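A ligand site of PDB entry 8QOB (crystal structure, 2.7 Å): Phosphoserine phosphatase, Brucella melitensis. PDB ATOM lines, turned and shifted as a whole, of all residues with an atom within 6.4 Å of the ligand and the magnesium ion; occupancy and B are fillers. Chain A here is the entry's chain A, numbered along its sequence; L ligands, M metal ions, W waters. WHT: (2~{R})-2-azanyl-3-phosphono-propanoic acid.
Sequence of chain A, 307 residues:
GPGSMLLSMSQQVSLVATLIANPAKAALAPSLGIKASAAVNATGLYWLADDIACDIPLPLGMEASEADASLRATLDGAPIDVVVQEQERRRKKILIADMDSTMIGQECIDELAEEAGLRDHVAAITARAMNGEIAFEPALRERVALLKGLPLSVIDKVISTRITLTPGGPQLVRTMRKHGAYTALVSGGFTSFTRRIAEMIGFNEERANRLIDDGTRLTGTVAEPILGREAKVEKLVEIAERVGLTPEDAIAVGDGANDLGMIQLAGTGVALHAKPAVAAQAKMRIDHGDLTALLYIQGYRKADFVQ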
ATOM      1  N   ASP A  98      30.809 -25.497 -20.889  1.00  0.00           N
ATOM      2  CA  ASP A  98      30.565 -24.461 -19.899  1.00  0.00           C
ATOM      3  C   ASP A  98      31.699 -24.408 -18.860  1.00  0.00           C
ATOM      4  O   ASP A  98      32.331 -25.412 -18.548  1.00  0.00           O
ATOM      5  CB  ASP A  98      29.258 -24.777 -19.204  1.00  0.00           C
ATOM      6  CG  ASP A  98      28.812 -23.664 -18.346  1.00  0.00           C
ATOM      7  OD1 ASP A  98      28.887 -22.504 -18.823  1.00  0.00           O
ATOM      8  OD2 ASP A  98      28.435 -23.952 -17.183  1.00  0.00           O
ATOM      9  N   MET A  99      31.949 -23.215 -18.318  1.00  0.00           N
ATOM     10  CA  MET A  99      32.898 -23.145 -17.199  1.00  0.00           C
ATOM     11  C   MET A  99      32.230 -23.254 -15.829  1.00  0.00           C
ATOM     12  O   MET A  99      32.317 -24.309 -15.193  1.00  0.00           O
ATOM     13  CB  MET A  99      33.742 -21.879 -17.261  1.00  0.00           C
ATOM     14  CG  MET A  99      35.027 -22.017 -16.445  1.00  0.00           C
ATOM     15  SD  MET A  99      35.815 -20.471 -15.906  1.00  0.00           S
ATOM     16  CE  MET A  99      34.409 -19.517 -15.307  1.00  0.00           C
ATOM     17  N   ASP A 100      31.596 -22.171 -15.376  1.00  0.00           N
ATOM     18  CA  ASP A 100      31.028 -22.106 -14.026  1.00  0.00           C
ATOM     19  C   ASP A 100      30.144 -23.310 -13.731  1.00  0.00           C
ATOM     20  O   ASP A 100      29.226 -23.616 -14.495  1.00  0.00           O
ATOM     21  CB  ASP A 100      30.204 -20.828 -13.864  1.00  0.00           C
ATOM     22  CG  ASP A 100      31.023 -19.641 -13.456  1.00  0.00           C
ATOM     23  OD1 ASP A 100      32.241 -19.800 -13.246  1.00  0.00           O
ATOM     24  OD2 ASP A 100      30.452 -18.547 -13.332  1.00  0.00           O
ATOM     25  N   SER A 101      30.426 -23.973 -12.612  1.00  0.00           N
ATOM     26  CA  SER A 101      29.697 -25.140 -12.095  1.00  0.00           C
ATOM     27  C   SER A 101      29.810 -26.390 -12.955  1.00  0.00           C
ATOM     28  O   SER A 101      29.358 -27.456 -12.540  1.00  0.00           O
ATOM     29  CB  SER A 101      28.201 -24.813 -11.896  1.00  0.00           C
ATOM     30  OG  SER A 101      27.999 -24.160 -10.661  1.00  0.00           O
ATOM     31  N   THR A 102      30.391 -26.299 -14.148  1.00  0.00           N
ATOM     32  CA  THR A 102      30.642 -27.487 -14.961  1.00  0.00           C
ATOM     33  C   THR A 102      32.086 -27.946 -14.855  1.00  0.00           C
ATOM     34  O   THR A 102      32.351 -29.086 -14.457  1.00  0.00           O
ATOM     35  CB  THR A 102      30.248 -27.239 -16.432  1.00  0.00           C
ATOM     36  OG1 THR A 102      28.826 -27.066 -16.528  1.00  0.00           O
ATOM     37  CG2 THR A 102      30.653 -28.418 -17.285  1.00  0.00           C
ATOM     38  N   GLU A 107      30.585 -20.729  -8.864  1.00  0.00           N
ATOM     39  CA  GLU A 107      30.110 -19.674  -9.746  1.00  0.00           C
ATOM     40  C   GLU A 107      31.026 -18.476  -9.534  1.00  0.00           C
ATOM     41  O   GLU A 107      31.044 -17.888  -8.440  1.00  0.00           O
ATOM     42  CB  GLU A 107      28.652 -19.304  -9.431  1.00  0.00           C
ATOM     43  CG  GLU A 107      27.679 -20.473  -9.566  1.00  0.00           C
ATOM     44  CD  GLU A 107      27.330 -20.786 -11.008  1.00  0.00           C
ATOM     45  OE1 GLU A 107      27.654 -19.964 -11.910  1.00  0.00           O
ATOM     46  OE2 GLU A 107      26.730 -21.852 -11.245  1.00  0.00           O
ATOM     47  N   CYS A 108      31.809 -18.130 -10.578  1.00  0.00           N
ATOM     48  CA  CYS A 108      32.776 -17.030 -10.484  1.00  0.00           C
ATOM     49  C   CYS A 108      32.083 -15.723 -10.073  1.00  0.00           C
ATOM     50  O   CYS A 108      32.640 -14.950  -9.293  1.00  0.00           O
ATOM     51  CB  CYS A 108      33.575 -16.883 -11.803  1.00  0.00           C
ATOM     52  SG  CYS A 108      32.809 -16.352 -13.457  1.00  0.00           S
ATOM     53  N   ILE A 109      30.864 -15.509 -10.553  1.00  0.00           N
ATOM     54  CA  ILE A 109      30.078 -14.327 -10.188  1.00  0.00           C
ATOM     55  C   ILE A 109      29.744 -14.337  -8.690  1.00  0.00           C
ATOM     56  O   ILE A 109      29.883 -13.308  -8.006  1.00  0.00           O
ATOM     57  CB  ILE A 109      28.825 -14.243 -11.087  1.00  0.00           C
ATOM     58  CG1 ILE A 109      27.962 -13.025 -10.751  1.00  0.00           C
ATOM     59  CG2 ILE A 109      28.027 -15.548 -11.028  1.00  0.00           C
ATOM     60  CD1 ILE A 109      28.635 -11.718 -10.966  1.00  0.00           C
ATOM     61  N   ASP A 110      29.324 -15.485  -8.149  1.00  0.00           N
ATOM     62  CA  ASP A 110      28.923 -15.586  -6.741  1.00  0.00           C
ATOM     63  C   ASP A 110      30.116 -15.408  -5.788  1.00  0.00           C
ATOM     64  O   ASP A 110      29.943 -14.955  -4.647  1.00  0.00           O
ATOM     65  CB  ASP A 110      28.259 -16.956  -6.466  1.00  0.00           C
ATOM     66  CG  ASP A 110      26.865 -17.094  -7.102  1.00  0.00           C
ATOM     67  OD1 ASP A 110      26.404 -16.142  -7.784  1.00  0.00           O
ATOM     68  OD2 ASP A 110      26.213 -18.152  -6.913  1.00  0.00           O
ATOM     69  N   THR A 126      21.759 -15.829  -9.393  1.00  0.00           N
ATOM     70  CA  THR A 126      22.442 -16.844 -10.197  1.00  0.00           C
ATOM     71  C   THR A 126      21.595 -18.108 -10.326  1.00  0.00           C
ATOM     72  O   THR A 126      21.376 -18.611 -11.427  1.00  0.00           O
ATOM     73  CB  THR A 126      23.796 -17.169  -9.577  1.00  0.00           C
ATOM     74  OG1 THR A 126      24.631 -16.006  -9.655  1.00  0.00           O
ATOM     75  CG2 THR A 126      24.472 -18.316 -10.322  1.00  0.00           C
ATOM     76  N   ALA A 129      18.736 -17.446 -12.693  1.00  0.00           N
ATOM     77  CA  ALA A 129      19.257 -17.352 -14.056  1.00  0.00           C
ATOM     78  C   ALA A 129      19.544 -18.736 -14.618  1.00  0.00           C
ATOM     79  O   ALA A 129      19.090 -19.089 -15.706  1.00  0.00           O
ATOM     80  CB  ALA A 129      20.523 -16.493 -14.078  1.00  0.00           C
ATOM     81  N   MET A 130      20.303 -19.541 -13.865  1.00  0.00           N
ATOM     82  CA  MET A 130      20.721 -20.830 -14.366  1.00  0.00           C
ATOM     83  C   MET A 130      19.577 -21.847 -14.428  1.00  0.00           C
ATOM     84  O   MET A 130      19.726 -22.877 -15.102  1.00  0.00           O
ATOM     85  CB  MET A 130      21.882 -21.354 -13.525  1.00  0.00           C
ATOM     86  CG  MET A 130      23.073 -20.386 -13.592  1.00  0.00           C
ATOM     87  SD  MET A 130      23.867 -20.438 -15.240  1.00  0.00           S
ATOM     88  CE  MET A 130      23.357 -18.818 -15.806  1.00  0.00           C
ATOM     89  N   PHE A 136      19.613 -14.458 -19.282  1.00  0.00           N
ATOM     90  CA  PHE A 136      20.971 -14.382 -18.752  1.00  0.00           C
ATOM     91  C   PHE A 136      21.463 -12.950 -18.677  1.00  0.00           C
ATOM     92  O   PHE A 136      22.136 -12.577 -17.707  1.00  0.00           O
ATOM     93  CB  PHE A 136      21.933 -15.206 -19.598  1.00  0.00           C
ATOM     94  CG  PHE A 136      23.323 -15.194 -19.058  1.00  0.00           C
ATOM     95  CD1 PHE A 136      23.649 -15.939 -17.926  1.00  0.00           C
ATOM     96  CD2 PHE A 136      24.297 -14.397 -19.651  1.00  0.00           C
ATOM     97  CE1 PHE A 136      24.934 -15.914 -17.403  1.00  0.00           C
ATOM     98  CE2 PHE A 136      25.600 -14.377 -19.141  1.00  0.00           C
ATOM     99  CZ  PHE A 136      25.923 -15.120 -18.023  1.00  0.00           C
ATOM    100  N   LEU A 140      23.114 -11.064 -15.592  1.00  0.00           N
ATOM    101  CA  LEU A 140      24.503 -10.638 -15.513  1.00  0.00           C
ATOM    102  C   LEU A 140      24.594  -9.175 -15.130  1.00  0.00           C
ATOM    103  O   LEU A 140      25.312  -8.812 -14.194  1.00  0.00           O
ATOM    104  CB  LEU A 140      25.221 -10.893 -16.835  1.00  0.00           C
ATOM    105  CG  LEU A 140      26.731 -10.946 -16.700  1.00  0.00           C
ATOM    106  CD1 LEU A 140      27.109 -11.873 -15.531  1.00  0.00           C
ATOM    107  CD2 LEU A 140      27.376 -11.434 -17.989  1.00  0.00           C
ATOM    108  N   ARG A 143      23.706  -8.612 -11.414  1.00  0.00           N
ATOM    109  CA  ARG A 143      24.700  -9.133 -10.484  1.00  0.00           C
ATOM    110  C   ARG A 143      26.021  -8.367 -10.587  1.00  0.00           C
ATOM    111  O   ARG A 143      26.600  -7.979  -9.571  1.00  0.00           O
ATOM    112  CB  ARG A 143      24.915 -10.630 -10.735  1.00  0.00           C
ATOM    113  CG  ARG A 143      23.751 -11.527 -10.279  1.00  0.00           C
ATOM    114  CD  ARG A 143      23.970 -12.955 -10.783  1.00  0.00           C
ATOM    115  NE  ARG A 143      23.858 -13.043 -12.238  1.00  0.00           N
ATOM    116  CZ  ARG A 143      24.177 -14.113 -12.949  1.00  0.00           C
ATOM    117  NH1 ARG A 143      24.716 -15.177 -12.385  1.00  0.00           N
ATOM    118  NH2 ARG A 143      23.944 -14.117 -14.259  1.00  0.00           N
ATOM    119  N   VAL A 186      33.587 -22.253 -23.190  1.00  0.00           N
ATOM    120  CA  VAL A 186      32.669 -21.194 -23.591  1.00  0.00           C
ATOM    121  C   VAL A 186      31.715 -20.891 -22.429  1.00  0.00           C
ATOM    122  O   VAL A 186      30.831 -21.699 -22.115  1.00  0.00           O
ATOM    123  CB  VAL A 186      31.903 -21.574 -24.873  1.00  0.00           C
ATOM    124  CG1 VAL A 186      31.038 -20.440 -25.338  1.00  0.00           C
ATOM    125  CG2 VAL A 186      32.919 -21.975 -25.941  1.00  0.00           C
ATOM    126  N   SER A 187      31.883 -19.702 -21.840  1.00  0.00           N
ATOM    127  CA  SER A 187      31.305 -19.326 -20.557  1.00  0.00           C
ATOM    128  C   SER A 187      30.563 -17.998 -20.691  1.00  0.00           C
ATOM    129  O   SER A 187      30.883 -17.155 -21.543  1.00  0.00           O
ATOM    130  CB  SER A 187      32.452 -19.237 -19.493  1.00  0.00           C
ATOM    131  OG  SER A 187      32.087 -18.587 -18.288  1.00  0.00           O
ATOM    132  N   GLY A 188      29.518 -17.832 -19.864  1.00  0.00           N
ATOM    133  CA  GLY A 188      28.905 -16.546 -19.629  1.00  0.00           C
ATOM    134  C   GLY A 188      29.580 -15.751 -18.540  1.00  0.00           C
ATOM    135  O   GLY A 188      29.117 -14.682 -18.142  1.00  0.00           O
ATOM    136  N   GLY A 189      30.696 -16.275 -18.042  1.00  0.00           N
ATOM    137  CA  GLY A 189      31.441 -15.640 -16.990  1.00  0.00           C
ATOM    138  C   GLY A 189      32.460 -14.687 -17.558  1.00  0.00           C
ATOM    139  O   GLY A 189      32.178 -14.005 -18.542  1.00  0.00           O
ATOM    140  N   PHE A 190      33.653 -14.621 -16.978  1.00  0.00           N
ATOM    141  CA  PHE A 190      34.519 -13.494 -17.254  1.00  0.00           C
ATOM    142  C   PHE A 190      35.883 -13.961 -17.749  1.00  0.00           C
ATOM    143  O   PHE A 190      36.436 -14.936 -17.238  1.00  0.00           O
ATOM    144  CB  PHE A 190      34.622 -12.626 -16.010  1.00  0.00           C
ATOM    145  CG  PHE A 190      33.267 -12.276 -15.449  1.00  0.00           C
ATOM    146  CD1 PHE A 190      32.385 -11.497 -16.180  1.00  0.00           C
ATOM    147  CD2 PHE A 190      32.853 -12.782 -14.221  1.00  0.00           C
ATOM    148  CE1 PHE A 190      31.123 -11.179 -15.697  1.00  0.00           C
ATOM    149  CE2 PHE A 190      31.577 -12.471 -13.721  1.00  0.00           C
ATOM    150  CZ  PHE A 190      30.721 -11.677 -14.456  1.00  0.00           C
ATOM    151  N   THR A 194      38.216 -17.369 -17.297  1.00  0.00           N
ATOM    152  CA  THR A 194      38.292 -18.441 -18.294  1.00  0.00           C
ATOM    153  C   THR A 194      39.678 -18.550 -18.913  1.00  0.00           C
ATOM    154  O   THR A 194      40.106 -19.664 -19.267  1.00  0.00           O
ATOM    155  CB  THR A 194      37.238 -18.211 -19.387  1.00  0.00           C
ATOM    156  OG1 THR A 194      37.400 -16.903 -19.959  1.00  0.00           O
ATOM    157  CG2 THR A 194      35.823 -18.391 -18.813  1.00  0.00           C
ATOM    158  N   LYS A 232      26.474 -18.795 -27.063  1.00  0.00           N
ATOM    159  CA  LYS A 232      27.103 -20.111 -26.968  1.00  0.00           C
ATOM    160  C   LYS A 232      26.791 -20.960 -28.199  1.00  0.00           C
ATOM    161  O   LYS A 232      27.640 -21.717 -28.663  1.00  0.00           O
ATOM    162  CB  LYS A 232      26.689 -20.828 -25.668  1.00  0.00           C
ATOM    163  CG  LYS A 232      27.293 -20.213 -24.404  1.00  0.00           C
ATOM    164  CD  LYS A 232      27.446 -21.210 -23.242  1.00  0.00           C
ATOM    165  CE  LYS A 232      27.409 -20.483 -21.875  1.00  0.00           C
ATOM    166  NZ  LYS A 232      28.367 -21.020 -20.860  1.00  0.00           N
ATOM    167  N   GLY A 254      27.031 -28.696 -20.175  1.00  0.00           N
ATOM    168  CA  GLY A 254      26.834 -27.598 -19.235  1.00  0.00           C
ATOM    169  C   GLY A 254      25.742 -27.982 -18.247  1.00  0.00           C
ATOM    170  O   GLY A 254      25.209 -29.093 -18.278  1.00  0.00           O
ATOM    171  N   ASP A 255      25.407 -27.017 -17.382  1.00  0.00           N
ATOM    172  CA  ASP A 255      24.501 -27.223 -16.256  1.00  0.00           C
ATOM    173  C   ASP A 255      23.303 -26.270 -16.224  1.00  0.00           C
ATOM    174  O   ASP A 255      22.321 -26.581 -15.541  1.00  0.00           O
ATOM    175  CB  ASP A 255      25.270 -27.049 -14.938  1.00  0.00           C
ATOM    176  CG  ASP A 255      25.653 -25.581 -14.656  1.00  0.00           C
ATOM    177  OD1 ASP A 255      26.359 -24.967 -15.488  1.00  0.00           O
ATOM    178  OD2 ASP A 255      25.244 -25.033 -13.599  1.00  0.00           O
ATOM    179  N   GLY A 256      23.370 -25.113 -16.898  1.00  0.00           N
ATOM    180  CA  GLY A 256      22.381 -24.085 -16.730  1.00  0.00           C
ATOM    181  C   GLY A 256      21.702 -23.782 -18.069  1.00  0.00           C
ATOM    182  O   GLY A 256      22.117 -24.280 -19.118  1.00  0.00           O
ATOM    183  N   ASN A 258      21.689 -21.293 -19.986  1.00  0.00           N
ATOM    184  CA  ASN A 258      22.475 -20.645 -21.043  1.00  0.00           C
ATOM    185  C   ASN A 258      23.262 -21.655 -21.869  1.00  0.00           C
ATOM    186  O   ASN A 258      23.887 -21.260 -22.862  1.00  0.00           O
ATOM    187  CB  ASN A 258      23.443 -19.600 -20.458  1.00  0.00           C
ATOM    188  CG  ASN A 258      24.216 -20.101 -19.256  1.00  0.00           C
ATOM    189  OD1 ASN A 258      23.721 -20.938 -18.488  1.00  0.00           O
ATOM    190  ND2 ASN A 258      25.445 -19.625 -19.096  1.00  0.00           N
ATOM    191  N   ASP A 259      23.293 -22.914 -21.470  1.00  0.00           N
ATOM    192  CA  ASP A 259      23.925 -23.969 -22.248  1.00  0.00           C
ATOM    193  C   ASP A 259      22.919 -24.754 -23.079  1.00  0.00           C
ATOM    194  O   ASP A 259      23.343 -25.617 -23.865  1.00  0.00           O
ATOM    195  CB  ASP A 259      24.704 -24.918 -21.334  1.00  0.00           C
ATOM    196  CG  ASP A 259      25.741 -24.197 -20.492  1.00  0.00           C
ATOM    197  OD1 ASP A 259      26.621 -23.543 -21.090  1.00  0.00           O
ATOM    198  OD2 ASP A 259      25.683 -24.318 -19.244  1.00  0.00           O
ATOM    199  N   LYS A 275      20.545 -28.074 -13.388  1.00  0.00           N
ATOM    200  CA  LYS A 275      19.481 -27.487 -12.614  1.00  0.00           C
ATOM    201  C   LYS A 275      18.140 -28.165 -12.947  1.00  0.00           C
ATOM    202  O   LYS A 275      17.983 -28.785 -14.017  1.00  0.00           O
ATOM    203  CB  LYS A 275      19.440 -25.972 -12.884  1.00  0.00           C
ATOM    204  CG  LYS A 275      20.346 -25.121 -11.960  1.00  0.00           C
ATOM    205  CD  LYS A 275      21.807 -25.420 -12.204  1.00  0.00           C
ATOM    206  CE  LYS A 275      22.746 -24.588 -11.328  1.00  0.00           C
ATOM    207  NZ  LYS A 275      23.952 -25.408 -10.977  1.00  0.00           N
HETATM  208  C01 WHT L   1      28.508 -18.383 -16.160  1.00  0.00           C
HETATM  209  C02 WHT L   1      27.601 -18.385 -14.879  1.00  0.00           C
HETATM  210  C03 WHT L   1      26.731 -17.124 -14.548  1.00  0.00           C
HETATM  211  N06 WHT L   1      26.782 -19.589 -14.775  1.00  0.00           N
HETATM  212  O04 WHT L   1      25.629 -17.206 -13.900  1.00  0.00           O
HETATM  213  O05 WHT L   1      27.097 -15.958 -14.874  1.00  0.00           O
HETATM  214  O08 WHT L   1      28.281 -21.188 -16.445  1.00  0.00           O
HETATM  215  O09 WHT L   1      28.127 -19.843 -18.500  1.00  0.00           O
HETATM  216  O10 WHT L   1      30.308 -20.350 -17.396  1.00  0.00           O
HETATM  217  P07 WHT L   1      28.851 -19.980 -17.155  1.00  0.00           P
HETATM  218 MG    MG M   1      27.377 -23.119 -15.593  1.00  0.00          MG
HETATM  219  O   HOH W   1      26.150 -22.678 -13.905  1.00  0.00           O
HETATM  220  O   HOH W   2      25.830 -22.784 -17.448  1.00  0.00           O
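The backbone NH of Asp 100 sits at hydrogen-bond distance from an oxygen (O10) of the ligand (3.0 Å). The side-chain amino group (NZ) of Lys 232 is in salt-bridge range of an oxygen (O09) of the ligand (2.6 Å). O10 of the ligand lies within hydrogen-bond range of OG of Ser 187 (2.7 Å). The guanidinium group (NH1) of Arg 143 is in salt-bridge range of an oxygen (O04) of the ligand, 2.7 Å away. The side-chain amide nitrogen (ND2) of Asn 258 lies within hydrogen-bond range of an oxygen (O09) of the ligand, 2.8 Å away. N of Gly 188 sits at hydrogen-bond distance from O09 of the ligand (2.8 Å). A nitrogen (N06) of the ligand lies within salt-bridge range of the side-chain carboxylate of Glu 107 (3.0 Å). SD of Met 130 sits at hydrogen-bond distance from N06 of the ligand (3.1 Å). N of Met 99 sits at hydrogen-bond distance from O10 of the ligand (3.4 Å).
The side-chain amino group of Lys 232 is in salt-bridge range of the side-chain carboxylate of Asp 98 (2.6 Å). The backbone NH (N) of Asp 255 sits at hydrogen-bond distance from the side-chain carboxylate (OD2) of Asp 259 (3.3 Å). The side-chain carboxylate (OD2) of Asp 255 is in salt-bridge range of the side-chain amino group (NZ) of Lys 275, at 2.9 Å. The side-chain carboxylate of Asp 100 sits at hydrogen-bond distance from the backbone NH of Cys 108 (3.1 Å). The side-chain amino group (NZ) of Lys 232 sits at hydrogen-bond distance from the backbone carbonyl oxygen (O) of Val 186, 2.8 Å away. OD1 of Asn 258 lies close to SD of Met 130 (3.3 Å). The side-chain carboxylate (OE2) of Glu 107 lies within hydrogen-bond range of the side-chain hydroxyl (OG) of Ser 101, at 2.7 Å. The side-chain hydroxyl (OG1) of Thr 126 sits at hydrogen-bond distance from the side-chain carboxylate (OD1) of Asp 110 (2.6 Å).
Residues that only touch the ligand: Phe 136, Gly 189, Thr 126 and Ile 109. Hydrophobic or aromatic side chains within 4 Å of the ligand: Met 99, Ile 109, Met 130 and Phe 136. Of the 28 residues printed, 14 come within 4 Å of the ligand.
Within 4 Å of the magnesium ion: Asp 98, Asp 100 and Asp 255. The nearest printed residue that does not touch the magnesium ion is Ser 101 (4.1 Å).
The magnesium ion is bound by OD2 of Asp 98, OD1 of Asp 255, water W1, O of Asp 100, O08 of the ligand and water W2. The magnesium ion has six donor atoms within binding distance.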
